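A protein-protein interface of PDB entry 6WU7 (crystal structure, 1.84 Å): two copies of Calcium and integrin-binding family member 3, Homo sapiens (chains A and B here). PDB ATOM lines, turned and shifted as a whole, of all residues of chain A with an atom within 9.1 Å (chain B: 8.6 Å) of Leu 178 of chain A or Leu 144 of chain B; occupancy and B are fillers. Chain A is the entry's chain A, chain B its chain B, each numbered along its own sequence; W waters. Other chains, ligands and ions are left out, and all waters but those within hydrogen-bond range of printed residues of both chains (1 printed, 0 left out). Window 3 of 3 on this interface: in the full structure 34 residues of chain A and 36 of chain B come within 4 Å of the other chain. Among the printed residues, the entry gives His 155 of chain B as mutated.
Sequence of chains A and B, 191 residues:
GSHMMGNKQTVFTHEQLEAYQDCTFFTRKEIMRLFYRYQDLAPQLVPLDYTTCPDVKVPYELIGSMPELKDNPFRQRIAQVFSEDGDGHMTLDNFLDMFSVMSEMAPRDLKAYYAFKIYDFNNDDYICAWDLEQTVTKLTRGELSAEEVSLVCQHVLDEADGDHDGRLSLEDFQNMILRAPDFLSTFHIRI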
ATOM      1  N   PRO A 107      -8.986  13.183  13.712  1.00  0.00           N
ATOM      2  CA  PRO A 107      -9.376  14.488  14.254  1.00  0.00           C
ATOM      3  C   PRO A 107     -10.142  14.367  15.558  1.00  0.00           C
ATOM      4  O   PRO A 107     -10.905  13.425  15.774  1.00  0.00           O
ATOM      5  CB  PRO A 107     -10.247  15.093  13.132  1.00  0.00           C
ATOM      6  CG  PRO A 107      -9.650  14.499  11.861  1.00  0.00           C
ATOM      7  CD  PRO A 107      -9.325  13.046  12.278  1.00  0.00           C
ATOM      8  N   ARG A 108      -9.955  15.382  16.417  1.00  0.00           N
ATOM      9  CA  ARG A 108     -10.600  15.390  17.725  1.00  0.00           C
ATOM     10  C   ARG A 108     -12.127  15.366  17.601  1.00  0.00           C
ATOM     11  O   ARG A 108     -12.805  14.712  18.385  1.00  0.00           O
ATOM     12  CB  ARG A 108     -10.167  16.640  18.508  1.00  0.00           C
ATOM     13  CG  ARG A 108     -10.282  16.532  20.051  1.00  0.00           C
ATOM     14  CD  ARG A 108      -9.337  17.549  20.788  1.00  0.00           C
ATOM     15  NE  ARG A 108      -9.794  17.833  22.155  1.00  0.00           N
ATOM     16  CZ  ARG A 108      -9.606  17.012  23.192  1.00  0.00           C
ATOM     17  NH1 ARG A 108     -10.069  17.355  24.396  1.00  0.00           N
ATOM     18  NH2 ARG A 108      -8.964  15.879  23.046  1.00  0.00           N
ATOM     19  N   ASP A 109     -12.684  16.098  16.646  1.00  0.00           N
ATOM     20  CA  ASP A 109     -14.150  16.093  16.499  1.00  0.00           C
ATOM     21  C   ASP A 109     -14.672  14.727  16.057  1.00  0.00           C
ATOM     22  O   ASP A 109     -15.832  14.379  16.337  1.00  0.00           O
ATOM     23  CB  ASP A 109     -14.537  17.200  15.521  1.00  0.00           C
ATOM     24  CG  ASP A 109     -16.003  17.613  15.634  1.00  0.00           C
ATOM     25  OD1 ASP A 109     -16.626  17.763  14.565  1.00  0.00           O
ATOM     26  OD2 ASP A 109     -16.492  17.833  16.766  1.00  0.00           O
ATOM     27  N   ALA A 112     -14.731  12.706  19.122  1.00  0.00           N
ATOM     28  CA  ALA A 112     -15.869  13.152  19.922  1.00  0.00           C
ATOM     29  C   ALA A 112     -17.169  12.542  19.430  1.00  0.00           C
ATOM     30  O   ALA A 112     -18.050  12.202  20.235  1.00  0.00           O
ATOM     31  CB  ALA A 112     -15.959  14.687  19.912  1.00  0.00           C
ATOM     32  N   LEU A 170     -25.870  14.830  20.493  1.00  0.00           N
ATOM     33  CA  LEU A 170     -24.555  14.687  19.859  1.00  0.00           C
ATOM     34  C   LEU A 170     -23.903  16.046  19.669  1.00  0.00           C
ATOM     35  O   LEU A 170     -22.695  16.225  19.906  1.00  0.00           O
ATOM     36  CB  LEU A 170     -24.711  13.984  18.527  1.00  0.00           C
ATOM     37  CG  LEU A 170     -23.504  13.899  17.601  1.00  0.00           C
ATOM     38  CD1 LEU A 170     -22.373  13.172  18.318  1.00  0.00           C
ATOM     39  CD2 LEU A 170     -23.919  13.205  16.333  1.00  0.00           C
ATOM     40  N   GLU A 171     -24.692  17.020  19.200  1.00  0.00           N
ATOM     41  CA  GLU A 171     -24.174  18.372  18.999  1.00  0.00           C
ATOM     42  C   GLU A 171     -23.765  19.007  20.321  1.00  0.00           C
ATOM     43  O   GLU A 171     -22.709  19.643  20.405  1.00  0.00           O
ATOM     44  CB  GLU A 171     -25.223  19.241  18.291  1.00  0.00           C
ATOM     45  CG  GLU A 171     -24.641  20.537  17.685  1.00  0.00           C
ATOM     46  CD  GLU A 171     -25.713  21.454  17.094  1.00  0.00           C
ATOM     47  OE1 GLU A 171     -26.852  21.428  17.588  1.00  0.00           O
ATOM     48  OE2 GLU A 171     -25.408  22.196  16.136  1.00  0.00           O
ATOM     49  N   ASP A 172     -24.611  18.884  21.362  1.00  0.00           N
ATOM     50  CA  ASP A 172     -24.230  19.391  22.687  1.00  0.00           C
ATOM     51  C   ASP A 172     -22.834  18.876  23.041  1.00  0.00           C
ATOM     52  O   ASP A 172     -21.935  19.635  23.450  1.00  0.00           O
ATOM     53  CB  ASP A 172     -25.200  18.927  23.790  1.00  0.00           C
ATOM     54  CG  ASP A 172     -26.549  19.664  23.797  1.00  0.00           C
ATOM     55  OD1 ASP A 172     -26.669  20.751  23.233  1.00  0.00           O
ATOM     56  OD2 ASP A 172     -27.498  19.119  24.419  1.00  0.00           O
ATOM     57  N   PHE A 173     -22.654  17.561  22.889  1.00  0.00           N
ATOM     58  CA  PHE A 173     -21.429  16.885  23.322  1.00  0.00           C
ATOM     59  C   PHE A 173     -20.228  17.289  22.476  1.00  0.00           C
ATOM     60  O   PHE A 173     -19.156  17.604  23.012  1.00  0.00           O
ATOM     61  CB  PHE A 173     -21.641  15.372  23.275  1.00  0.00           C
ATOM     62  CG  PHE A 173     -20.462  14.574  23.780  1.00  0.00           C
ATOM     63  CD1 PHE A 173     -20.304  14.336  25.129  1.00  0.00           C
ATOM     64  CD2 PHE A 173     -19.534  14.082  22.906  1.00  0.00           C
ATOM     65  CE1 PHE A 173     -19.214  13.618  25.595  1.00  0.00           C
ATOM     66  CE2 PHE A 173     -18.433  13.357  23.361  1.00  0.00           C
ATOM     67  CZ  PHE A 173     -18.271  13.127  24.697  1.00  0.00           C
ATOM     68  N   GLN A 174     -20.361  17.241  21.148  1.00  0.00           N
ATOM     69  CA  GLN A 174     -19.215  17.579  20.305  1.00  0.00           C
ATOM     70  C   GLN A 174     -18.767  19.023  20.533  1.00  0.00           C
ATOM     71  O   GLN A 174     -17.566  19.334  20.484  1.00  0.00           O
ATOM     72  CB  GLN A 174     -19.546  17.365  18.833  1.00  0.00           C
ATOM     73  CG  GLN A 174     -19.727  15.911  18.401  1.00  0.00           C
ATOM     74  CD  GLN A 174     -19.835  15.768  16.890  1.00  0.00           C
ATOM     75  OE1 GLN A 174     -20.890  16.022  16.302  1.00  0.00           O
ATOM     76  NE2 GLN A 174     -18.735  15.369  16.249  1.00  0.00           N
ATOM     77  N   ASN A 175     -19.720  19.932  20.745  1.00  0.00           N
ATOM     78  CA  ASN A 175     -19.337  21.323  20.966  1.00  0.00           C
ATOM     79  C   ASN A 175     -18.713  21.516  22.347  1.00  0.00           C
ATOM     80  O   ASN A 175     -17.817  22.356  22.497  1.00  0.00           O
ATOM     81  CB  ASN A 175     -20.553  22.231  20.754  1.00  0.00           C
ATOM     82  CG  ASN A 175     -20.888  22.412  19.266  1.00  0.00           C
ATOM     83  OD1 ASN A 175     -20.076  22.092  18.389  1.00  0.00           O
ATOM     84  ND2 ASN A 175     -22.062  22.958  18.979  1.00  0.00           N
ATOM     85  N   MET A 176     -19.119  20.723  23.346  1.00  0.00           N
ATOM     86  CA  MET A 176     -18.440  20.767  24.646  1.00  0.00           C
ATOM     87  C   MET A 176     -16.966  20.378  24.502  1.00  0.00           C
ATOM     88  O   MET A 176     -16.077  21.002  25.102  1.00  0.00           O
ATOM     89  CB  MET A 176     -19.146  19.850  25.656  1.00  0.00           C
ATOM     90  CG  MET A 176     -18.359  19.512  26.951  1.00  0.00           C
ATOM     91  SD  MET A 176     -19.225  18.298  28.020  1.00  0.00           S
ATOM     92  CE  MET A 176     -18.522  16.819  27.312  1.00  0.00           C
ATOM     93  N   ILE A 177     -16.704  19.312  23.749  1.00  0.00           N
ATOM     94  CA  ILE A 177     -15.332  18.867  23.516  1.00  0.00           C
ATOM     95  C   ILE A 177     -14.557  19.916  22.734  1.00  0.00           C
ATOM     96  O   ILE A 177     -13.387  20.180  23.028  1.00  0.00           O
ATOM     97  CB  ILE A 177     -15.342  17.533  22.764  1.00  0.00           C
ATOM     98  CG1 ILE A 177     -16.060  16.427  23.559  1.00  0.00           C
ATOM     99  CG2 ILE A 177     -13.921  17.079  22.457  1.00  0.00           C
ATOM    100  CD1 ILE A 177     -15.445  16.170  24.888  1.00  0.00           C
ATOM    101  N   LEU A 178     -15.181  20.486  21.692  1.00  0.00           N
ATOM    102  CA  LEU A 178     -14.529  21.512  20.886  1.00  0.00           C
ATOM    103  C   LEU A 178     -14.059  22.678  21.750  1.00  0.00           C
ATOM    104  O   LEU A 178     -13.000  23.262  21.497  1.00  0.00           O
ATOM    105  CB  LEU A 178     -15.500  21.994  19.799  1.00  0.00           C
ATOM    106  CG  LEU A 178     -15.107  23.172  18.901  1.00  0.00           C
ATOM    107  CD1 LEU A 178     -13.930  22.856  18.031  1.00  0.00           C
ATOM    108  CD2 LEU A 178     -16.311  23.549  18.015  1.00  0.00           C
ATOM    109  N   ARG A 179     -14.831  23.035  22.772  1.00  0.00           N
ATOM    110  CA  ARG A 179     -14.476  24.168  23.616  1.00  0.00           C
ATOM    111  C   ARG A 179     -13.473  23.804  24.704  1.00  0.00           C
ATOM    112  O   ARG A 179     -13.091  24.693  25.478  1.00  0.00           O
ATOM    113  CB  ARG A 179     -15.738  24.764  24.246  1.00  0.00           C
ATOM    114  CG  ARG A 179     -16.630  25.474  23.204  1.00  0.00           C
ATOM    115  CD  ARG A 179     -17.833  26.150  23.816  1.00  0.00           C
ATOM    116  NE  ARG A 179     -18.614  25.213  24.600  1.00  0.00           N
ATOM    117  CZ  ARG A 179     -19.786  24.710  24.224  1.00  0.00           C
ATOM    118  NH1 ARG A 179     -20.415  23.848  25.014  1.00  0.00           N
ATOM    119  NH2 ARG A 179     -20.323  25.064  23.059  1.00  0.00           N
ATOM    120  N   ALA A 180     -13.012  22.559  24.753  1.00  0.00           N
ATOM    121  CA  ALA A 180     -12.139  22.076  25.826  1.00  0.00           C
ATOM    122  C   ALA A 180     -10.925  21.377  25.233  1.00  0.00           C
ATOM    123  O   ALA A 180     -10.821  20.144  25.251  1.00  0.00           O
ATOM    124  CB  ALA A 180     -12.917  21.134  26.745  1.00  0.00           C
ATOM    125  N   PRO A 181      -9.970  22.132  24.702  1.00  0.00           N
ATOM    126  CA  PRO A 181      -8.766  21.495  24.142  1.00  0.00           C
ATOM    127  C   PRO A 181      -7.974  20.752  25.211  1.00  0.00           C
ATOM    128  O   PRO A 181      -8.138  20.972  26.410  1.00  0.00           O
ATOM    129  CB  PRO A 181      -7.951  22.668  23.573  1.00  0.00           C
ATOM    130  CG  PRO A 181      -8.801  23.891  23.701  1.00  0.00           C
ATOM    131  CD  PRO A 181      -9.972  23.599  24.580  1.00  0.00           C
ATOM    132  N   ASP A 182      -7.139  19.823  24.756  1.00  0.00           N
ATOM    133  CA  ASP A 182      -6.348  18.962  25.648  1.00  0.00           C
ATOM    134  C   ASP A 182      -5.026  19.665  25.937  1.00  0.00           C
ATOM    135  O   ASP A 182      -3.996  19.430  25.308  1.00  0.00           O
ATOM    136  CB  ASP A 182      -6.112  17.592  25.035  1.00  0.00           C
ATOM    137  CG  ASP A 182      -5.485  16.623  26.003  1.00  0.00           C
ATOM    138  OD1 ASP A 182      -5.025  17.045  27.089  1.00  0.00           O
ATOM    139  OD2 ASP A 182      -5.402  15.433  25.654  1.00  0.00           O
ATOM    140  N   PHE A 183      -5.075  20.543  26.927  1.00  0.00           N
ATOM    141  CA  PHE A 183      -3.910  21.354  27.251  1.00  0.00           C
ATOM    142  C   PHE A 183      -2.755  20.533  27.813  1.00  0.00           C
ATOM    143  O   PHE A 183      -1.619  21.016  27.789  1.00  0.00           O
ATOM    144  CB  PHE A 183      -4.277  22.431  28.256  1.00  0.00           C
ATOM    145  CG  PHE A 183      -5.122  23.523  27.669  1.00  0.00           C
ATOM    146  CD1 PHE A 183      -4.539  24.496  26.887  1.00  0.00           C
ATOM    147  CD2 PHE A 183      -6.479  23.549  27.883  1.00  0.00           C
ATOM    148  CE1 PHE A 183      -5.294  25.513  26.334  1.00  0.00           C
ATOM    149  CE2 PHE A 183      -7.268  24.559  27.306  1.00  0.00           C
ATOM    150  CZ  PHE A 183      -6.663  25.544  26.547  1.00  0.00           C
ATOM    151  N   VAL B 136      -3.773  27.387  21.413  1.00  0.00           N
ATOM    152  CA  VAL B 136      -4.855  26.574  20.862  1.00  0.00           C
ATOM    153  C   VAL B 136      -4.632  26.330  19.378  1.00  0.00           C
ATOM    154  O   VAL B 136      -4.984  25.256  18.860  1.00  0.00           O
ATOM    155  CB  VAL B 136      -6.197  27.251  21.154  1.00  0.00           C
ATOM    156  CG1 VAL B 136      -7.316  26.565  20.367  1.00  0.00           C
ATOM    157  CG2 VAL B 136      -6.480  27.245  22.644  1.00  0.00           C
ATOM    158  N   THR B 137      -4.065  27.301  18.666  1.00  0.00           N
ATOM    159  CA  THR B 137      -3.754  27.093  17.254  1.00  0.00           C
ATOM    160  C   THR B 137      -2.816  25.910  17.103  1.00  0.00           C
ATOM    161  O   THR B 137      -3.007  25.049  16.236  1.00  0.00           O
ATOM    162  CB  THR B 137      -3.142  28.354  16.664  1.00  0.00           C
ATOM    163  OG1 THR B 137      -4.106  29.424  16.688  1.00  0.00           O
ATOM    164  CG2 THR B 137      -2.699  28.139  15.229  1.00  0.00           C
ATOM    165  N   LEU B 139      -2.291  23.407  19.364  1.00  0.00           N
ATOM    166  CA  LEU B 139      -2.874  22.159  19.829  1.00  0.00           C
ATOM    167  C   LEU B 139      -3.864  21.574  18.824  1.00  0.00           C
ATOM    168  O   LEU B 139      -4.045  20.351  18.787  1.00  0.00           O
ATOM    169  CB  LEU B 139      -3.578  22.356  21.169  1.00  0.00           C
ATOM    170  CG  LEU B 139      -2.742  22.513  22.434  1.00  0.00           C
ATOM    171  CD1 LEU B 139      -3.640  23.046  23.549  1.00  0.00           C
ATOM    172  CD2 LEU B 139      -2.119  21.206  22.802  1.00  0.00           C
ATOM    173  N   THR B 140      -4.547  22.405  18.055  1.00  0.00           N
ATOM    174  CA  THR B 140      -5.584  21.872  17.177  1.00  0.00           C
ATOM    175  C   THR B 140      -5.076  21.571  15.776  1.00  0.00           C
ATOM    176  O   THR B 140      -5.794  20.926  15.001  1.00  0.00           O
ATOM    177  CB  THR B 140      -6.788  22.820  17.132  1.00  0.00           C
ATOM    178  OG1 THR B 140      -6.388  24.117  16.711  1.00  0.00           O
ATOM    179  CG2 THR B 140      -7.403  22.900  18.543  1.00  0.00           C
ATOM    180  N   ARG B 141      -3.847  21.986  15.454  1.00  0.00           N
ATOM    181  CA  ARG B 141      -3.114  21.486  14.283  1.00  0.00           C
ATOM    182  C   ARG B 141      -3.874  21.667  12.976  1.00  0.00           C
ATOM    183  O   ARG B 141      -3.776  20.848  12.057  1.00  0.00           O
ATOM    184  CB  ARG B 141      -2.744  20.019  14.479  1.00  0.00           C
ATOM    185  CG  ARG B 141      -1.683  19.851  15.527  1.00  0.00           C
ATOM    186  CD  ARG B 141      -0.893  18.602  15.288  1.00  0.00           C
ATOM    187  NE  ARG B 141      -1.730  17.434  15.530  1.00  0.00           N
ATOM    188  CZ  ARG B 141      -1.270  16.197  15.649  1.00  0.00           C
ATOM    189  NH1 ARG B 141       0.040  15.957  15.547  1.00  0.00           N
ATOM    190  NH2 ARG B 141      -2.122  15.205  15.873  1.00  0.00           N
ATOM    191  N   GLY B 142      -4.575  22.779  12.856  1.00  0.00           N
ATOM    192  CA  GLY B 142      -5.284  23.076  11.645  1.00  0.00           C
ATOM    193  C   GLY B 142      -6.671  22.492  11.573  1.00  0.00           C
ATOM    194  O   GLY B 142      -7.372  22.727  10.583  1.00  0.00           O
ATOM    195  N   GLU B 143      -7.093  21.732  12.590  1.00  0.00           N
ATOM    196  CA  GLU B 143      -8.426  21.144  12.547  1.00  0.00           C
ATOM    197  C   GLU B 143      -9.503  22.209  12.690  1.00  0.00           C
ATOM    198  O   GLU B 143     -10.624  22.022  12.210  1.00  0.00           O
ATOM    199  CB  GLU B 143      -8.574  20.109  13.650  1.00  0.00           C
ATOM    200  CG  GLU B 143      -7.593  18.939  13.508  1.00  0.00           C
ATOM    201  CD  GLU B 143      -7.689  17.887  14.582  1.00  0.00           C
ATOM    202  OE1 GLU B 143      -8.745  17.819  15.275  1.00  0.00           O
ATOM    203  OE2 GLU B 143      -6.695  17.102  14.701  1.00  0.00           O
ATOM    204  N   LEU B 144      -9.187  23.311  13.357  1.00  0.00           N
ATOM    205  CA  LEU B 144     -10.089  24.442  13.513  1.00  0.00           C
ATOM    206  C   LEU B 144      -9.670  25.601  12.617  1.00  0.00           C
ATOM    207  O   LEU B 144      -8.481  25.839  12.383  1.00  0.00           O
ATOM    208  CB  LEU B 144     -10.093  24.900  14.966  1.00  0.00           C
ATOM    209  CG  LEU B 144     -10.637  23.919  15.997  1.00  0.00           C
ATOM    210  CD1 LEU B 144     -10.497  24.599  17.361  1.00  0.00           C
ATOM    211  CD2 LEU B 144     -12.045  23.521  15.656  1.00  0.00           C
ATOM    212  N   SER B 145     -10.664  26.331  12.124  1.00  0.00           N
ATOM    213  CA  SER B 145     -10.407  27.597  11.460  1.00  0.00           C
ATOM    214  C   SER B 145      -9.905  28.631  12.461  1.00  0.00           C
ATOM    215  O   SER B 145     -10.039  28.485  13.684  1.00  0.00           O
ATOM    216  CB  SER B 145     -11.670  28.123  10.799  1.00  0.00           C
ATOM    217  OG  SER B 145     -12.648  28.442  11.784  1.00  0.00           O
ATOM    218  N   ALA B 146      -9.334  29.707  11.921  1.00  0.00           N
ATOM    219  CA  ALA B 146      -8.916  30.809  12.778  1.00  0.00           C
ATOM    220  C   ALA B 146     -10.099  31.374  13.561  1.00  0.00           C
ATOM    221  O   ALA B 146      -9.967  31.737  14.734  1.00  0.00           O
ATOM    222  CB  ALA B 146      -8.282  31.908  11.919  1.00  0.00           C
ATOM    223  N   GLU B 147     -11.255  31.481  12.909  1.00  0.00           N
ATOM    224  CA  GLU B 147     -12.457  31.959  13.575  1.00  0.00           C
ATOM    225  C   GLU B 147     -12.843  31.042  14.734  1.00  0.00           C
ATOM    226  O   GLU B 147     -13.184  31.507  15.831  1.00  0.00           O
ATOM    227  CB  GLU B 147     -13.600  32.041  12.555  1.00  0.00           C
ATOM    228  CG  GLU B 147     -13.415  33.012  11.350  1.00  0.00           C
ATOM    229  CD  GLU B 147     -12.128  32.835  10.534  1.00  0.00           C
ATOM    230  OE1 GLU B 147     -11.765  31.692  10.170  1.00  0.00           O
ATOM    231  OE2 GLU B 147     -11.473  33.863  10.243  1.00  0.00           O
ATOM    232  N   GLU B 148     -12.820  29.723  14.497  1.00  0.00           N
ATOM    233  CA  GLU B 148     -13.164  28.764  15.545  1.00  0.00           C
ATOM    234  C   GLU B 148     -12.160  28.830  16.687  1.00  0.00           C
ATOM    235  O   GLU B 148     -12.544  28.780  17.863  1.00  0.00           O
ATOM    236  CB  GLU B 148     -13.227  27.343  14.960  1.00  0.00           C
ATOM    237  CG  GLU B 148     -14.529  27.028  14.222  1.00  0.00           C
ATOM    238  CD  GLU B 148     -14.484  25.761  13.380  1.00  0.00           C
ATOM    239  OE1 GLU B 148     -13.395  25.327  12.958  1.00  0.00           O
ATOM    240  OE2 GLU B 148     -15.562  25.181  13.142  1.00  0.00           O
ATOM    241  N   VAL B 149     -10.868  28.966  16.366  1.00  0.00           N
ATOM    242  CA  VAL B 149      -9.863  29.085  17.431  1.00  0.00           C
ATOM    243  C   VAL B 149     -10.162  30.290  18.313  1.00  0.00           C
ATOM    244  O   VAL B 149     -10.100  30.206  19.545  1.00  0.00           O
ATOM    245  CB  VAL B 149      -8.448  29.171  16.838  1.00  0.00           C
ATOM    246  CG1 VAL B 149      -7.479  29.716  17.884  1.00  0.00           C
ATOM    247  CG2 VAL B 149      -8.001  27.815  16.359  1.00  0.00           C
ATOM    248  N   SER B 150     -10.449  31.440  17.696  1.00  0.00           N
ATOM    249  CA  SER B 150     -10.768  32.632  18.476  1.00  0.00           C
ATOM    250  C   SER B 150     -11.974  32.410  19.371  1.00  0.00           C
ATOM    251  O   SER B 150     -11.975  32.827  20.536  1.00  0.00           O
ATOM    252  CB  SER B 150     -11.026  33.828  17.559  1.00  0.00           C
ATOM    253  OG  SER B 150      -9.868  34.176  16.837  1.00  0.00           O
ATOM    254  N   LEU B 151     -13.018  31.766  18.845  1.00  0.00           N
ATOM    255  CA  LEU B 151     -14.200  31.523  19.663  1.00  0.00           C
ATOM    256  C   LEU B 151     -13.875  30.592  20.818  1.00  0.00           C
ATOM    257  O   LEU B 151     -14.374  30.785  21.928  1.00  0.00           O
ATOM    258  CB  LEU B 151     -15.336  30.946  18.820  1.00  0.00           C
ATOM    259  CG  LEU B 151     -16.013  31.969  17.900  1.00  0.00           C
ATOM    260  CD1 LEU B 151     -16.785  31.293  16.770  1.00  0.00           C
ATOM    261  CD2 LEU B 151     -16.930  32.916  18.689  1.00  0.00           C
ATOM    262  N   VAL B 152     -13.030  29.583  20.584  1.00  0.00           N
ATOM    263  CA  VAL B 152     -12.658  28.663  21.656  1.00  0.00           C
ATOM    264  C   VAL B 152     -11.826  29.379  22.720  1.00  0.00           C
ATOM    265  O   VAL B 152     -12.035  29.183  23.924  1.00  0.00           O
ATOM    266  CB  VAL B 152     -11.913  27.447  21.066  1.00  0.00           C
ATOM    267  CG1 VAL B 152     -11.235  26.635  22.177  1.00  0.00           C
ATOM    268  CG2 VAL B 152     -12.860  26.583  20.263  1.00  0.00           C
ATOM    269  N   CYS B 153     -10.888  30.233  22.302  1.00  0.00           N
ATOM    270  CA  CYS B 153     -10.050  30.948  23.263  1.00  0.00           C
ATOM    271  C   CYS B 153     -10.879  31.899  24.118  1.00  0.00           C
ATOM    272  O   CYS B 153     -10.644  32.017  25.327  1.00  0.00           O
ATOM    273  CB  CYS B 153      -8.947  31.728  22.546  1.00  0.00           C
ATOM    274  SG  CYS B 153      -7.745  30.616  21.787  1.00  0.00           S
ATOM    275  N   HIS B 155     -13.981  31.480  24.935  1.00  0.00           N
ATOM    276  CA  HIS B 155     -14.741  30.659  25.876  1.00  0.00           C
ATOM    277  C   HIS B 155     -13.848  30.185  27.012  1.00  0.00           C
ATOM    278  O   HIS B 155     -14.224  30.249  28.192  1.00  0.00           O
ATOM    279  CB  HIS B 155     -15.355  29.447  25.175  1.00  0.00           C
ATOM    280  CG  HIS B 155     -16.040  28.497  26.111  1.00  0.00           C
ATOM    281  ND1 HIS B 155     -17.358  28.630  26.471  1.00  0.00           N
ATOM    282  CD2 HIS B 155     -15.577  27.418  26.786  1.00  0.00           C
ATOM    283  CE1 HIS B 155     -17.688  27.660  27.308  1.00  0.00           C
ATOM    284  NE2 HIS B 155     -16.624  26.910  27.519  1.00  0.00           N
ATOM    285  N   VAL B 156     -12.663  29.683  26.664  1.00  0.00           N
ATOM    286  CA  VAL B 156     -11.730  29.182  27.675  1.00  0.00           C
ATOM    287  C   VAL B 156     -11.450  30.261  28.704  1.00  0.00           C
ATOM    288  O   VAL B 156     -11.509  30.028  29.918  1.00  0.00           O
ATOM    289  CB  VAL B 156     -10.436  28.689  27.006  1.00  0.00           C
ATOM    290  CG1 VAL B 156      -9.371  28.489  28.071  1.00  0.00           C
ATOM    291  CG2 VAL B 156     -10.675  27.390  26.260  1.00  0.00           C
ATOM    292  N   LEU B 184     -12.051  12.705  26.275  1.00  0.00           N
ATOM    293  CA  LEU B 184     -11.459  11.990  25.147  1.00  0.00           C
ATOM    294  C   LEU B 184     -10.210  11.229  25.543  1.00  0.00           C
ATOM    295  O   LEU B 184      -9.574  10.616  24.677  1.00  0.00           O
ATOM    296  CB  LEU B 184     -11.124  12.950  24.002  1.00  0.00           C
ATOM    297  CG  LEU B 184     -12.247  13.520  23.121  1.00  0.00           C
ATOM    298  CD1 LEU B 184     -11.604  14.171  21.908  1.00  0.00           C
ATOM    299  CD2 LEU B 184     -13.247  12.486  22.734  1.00  0.00           C
HETATM  300  O   HOH W   1     -11.317  18.021  14.939  1.00  0.00           O
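The backbone NH (N) of Arg 108 of chain A sits at hydrogen-bond distance from the side-chain carboxylate (OE1) of Glu 143 of chain B (3.0 Å).
Water W1 lies within hydrogen-bond range of the side-chain carboxylate of Glu 143 of chain B, the backbone NH of Asp 109 of chain A and the backbone NH of Arg 108 of chain A.
Glu 171 of chain A touches none of the printed residues of chain B. Met 176 of chain A touches none of the printed residues of chain B. Of chain B, only Leu 144 (3.1 Å) and Val 152 (3.5 Å) come within 4 Å of Leu 178 of chain A. Of the printed residues of chain A, Leu 139 of chain B touches Asp 182 (3.6 Å) and Phe 183 (3.7 Å). No residue of chain A comes within 4 Å of Gly 142 of chain B. Printed residues of chain A within 4 Å of Glu 143 of chain B: Pro 107 (3.5 Å) and Arg 108 (3.0 Å). Leu 144 of chain B touches just one residue of chain A: Leu 178. No residue of chain A comes within 4 Å of Ser 145 of chain B. Printed residues of chain A within 4 Å of Val 152 of chain B: Leu 178 and Pro 181. Printed residues of chain A within 4 Å of His 155 of chain B: Arg 179 (3.7 Å). Of the printed residues of chain A, Leu 184 of chain B touches Arg 108 (3.3 Å), Ala 112 (3.9 Å) and Ile 177 (3.8 Å). The nearest residue of chain A that does not touch Leu 144 of chain B is Pro 181 of chain A (6.6 Å). The nearest printed residue of chain A that does not touch Val 156 of chain B is Pro 181 of chain A (4.2 Å).
The guanidinium group (NH1) of Arg 108 of chain A lies within hydrogen-bond range of the backbone carbonyl oxygen (O) of Ala 180 of chain A, at 3.0 Å.
Hydrophobic or aromatic side chains of chain B within 4 Å of the printed part of chain A: Leu 139, Leu 144, Val 152, His 155, Val 156 and Leu 184. Printed residues of chain A that touch a printed residue of chain B: Pro 107, Arg 108, Ala 112, Ile 177, Leu 178, Arg 179, Pro 181, Asp 182 and Phe 183. Among the printed residues, no Asp or Glu carboxylate lies within 4 Å of a Lys or Arg side-chain nitrogen of the other chain.
Pro 107 of chain A touches Glu 143 of chain B. Arg 108 of chain A touches Leu 184 of chain B (CG to CD1, 3.3 Å). Ile 177 of chain A touches Leu 184 of chain B (CG2 to CD1, 3.8 Å). Leu 144 of chain B touches Leu 178 of chain A. CG2 of Val 152 of chain B touches O of Leu 178 of chain A, 3.5 Å away. Arg 179 of chain A touches His 155 of chain B (CD to ND1, 3.7 Å). Arg 179 of chain A touches Val 156 of chain B (O to CG2, 3.7 Å). Val 152 of chain B touches Pro 181 of chain A (CG1 to CG, 3.97 Å). Leu 139 of chain B touches Asp 182 of chain A (CD2 to O, 3.6 Å). Phe 183 of chain A touches Leu 139 of chain B.
No position is printed for both chains. Of the 12 pairs that touch across the chains among the printed residues, none has its exchanged pair printed and touching as well.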
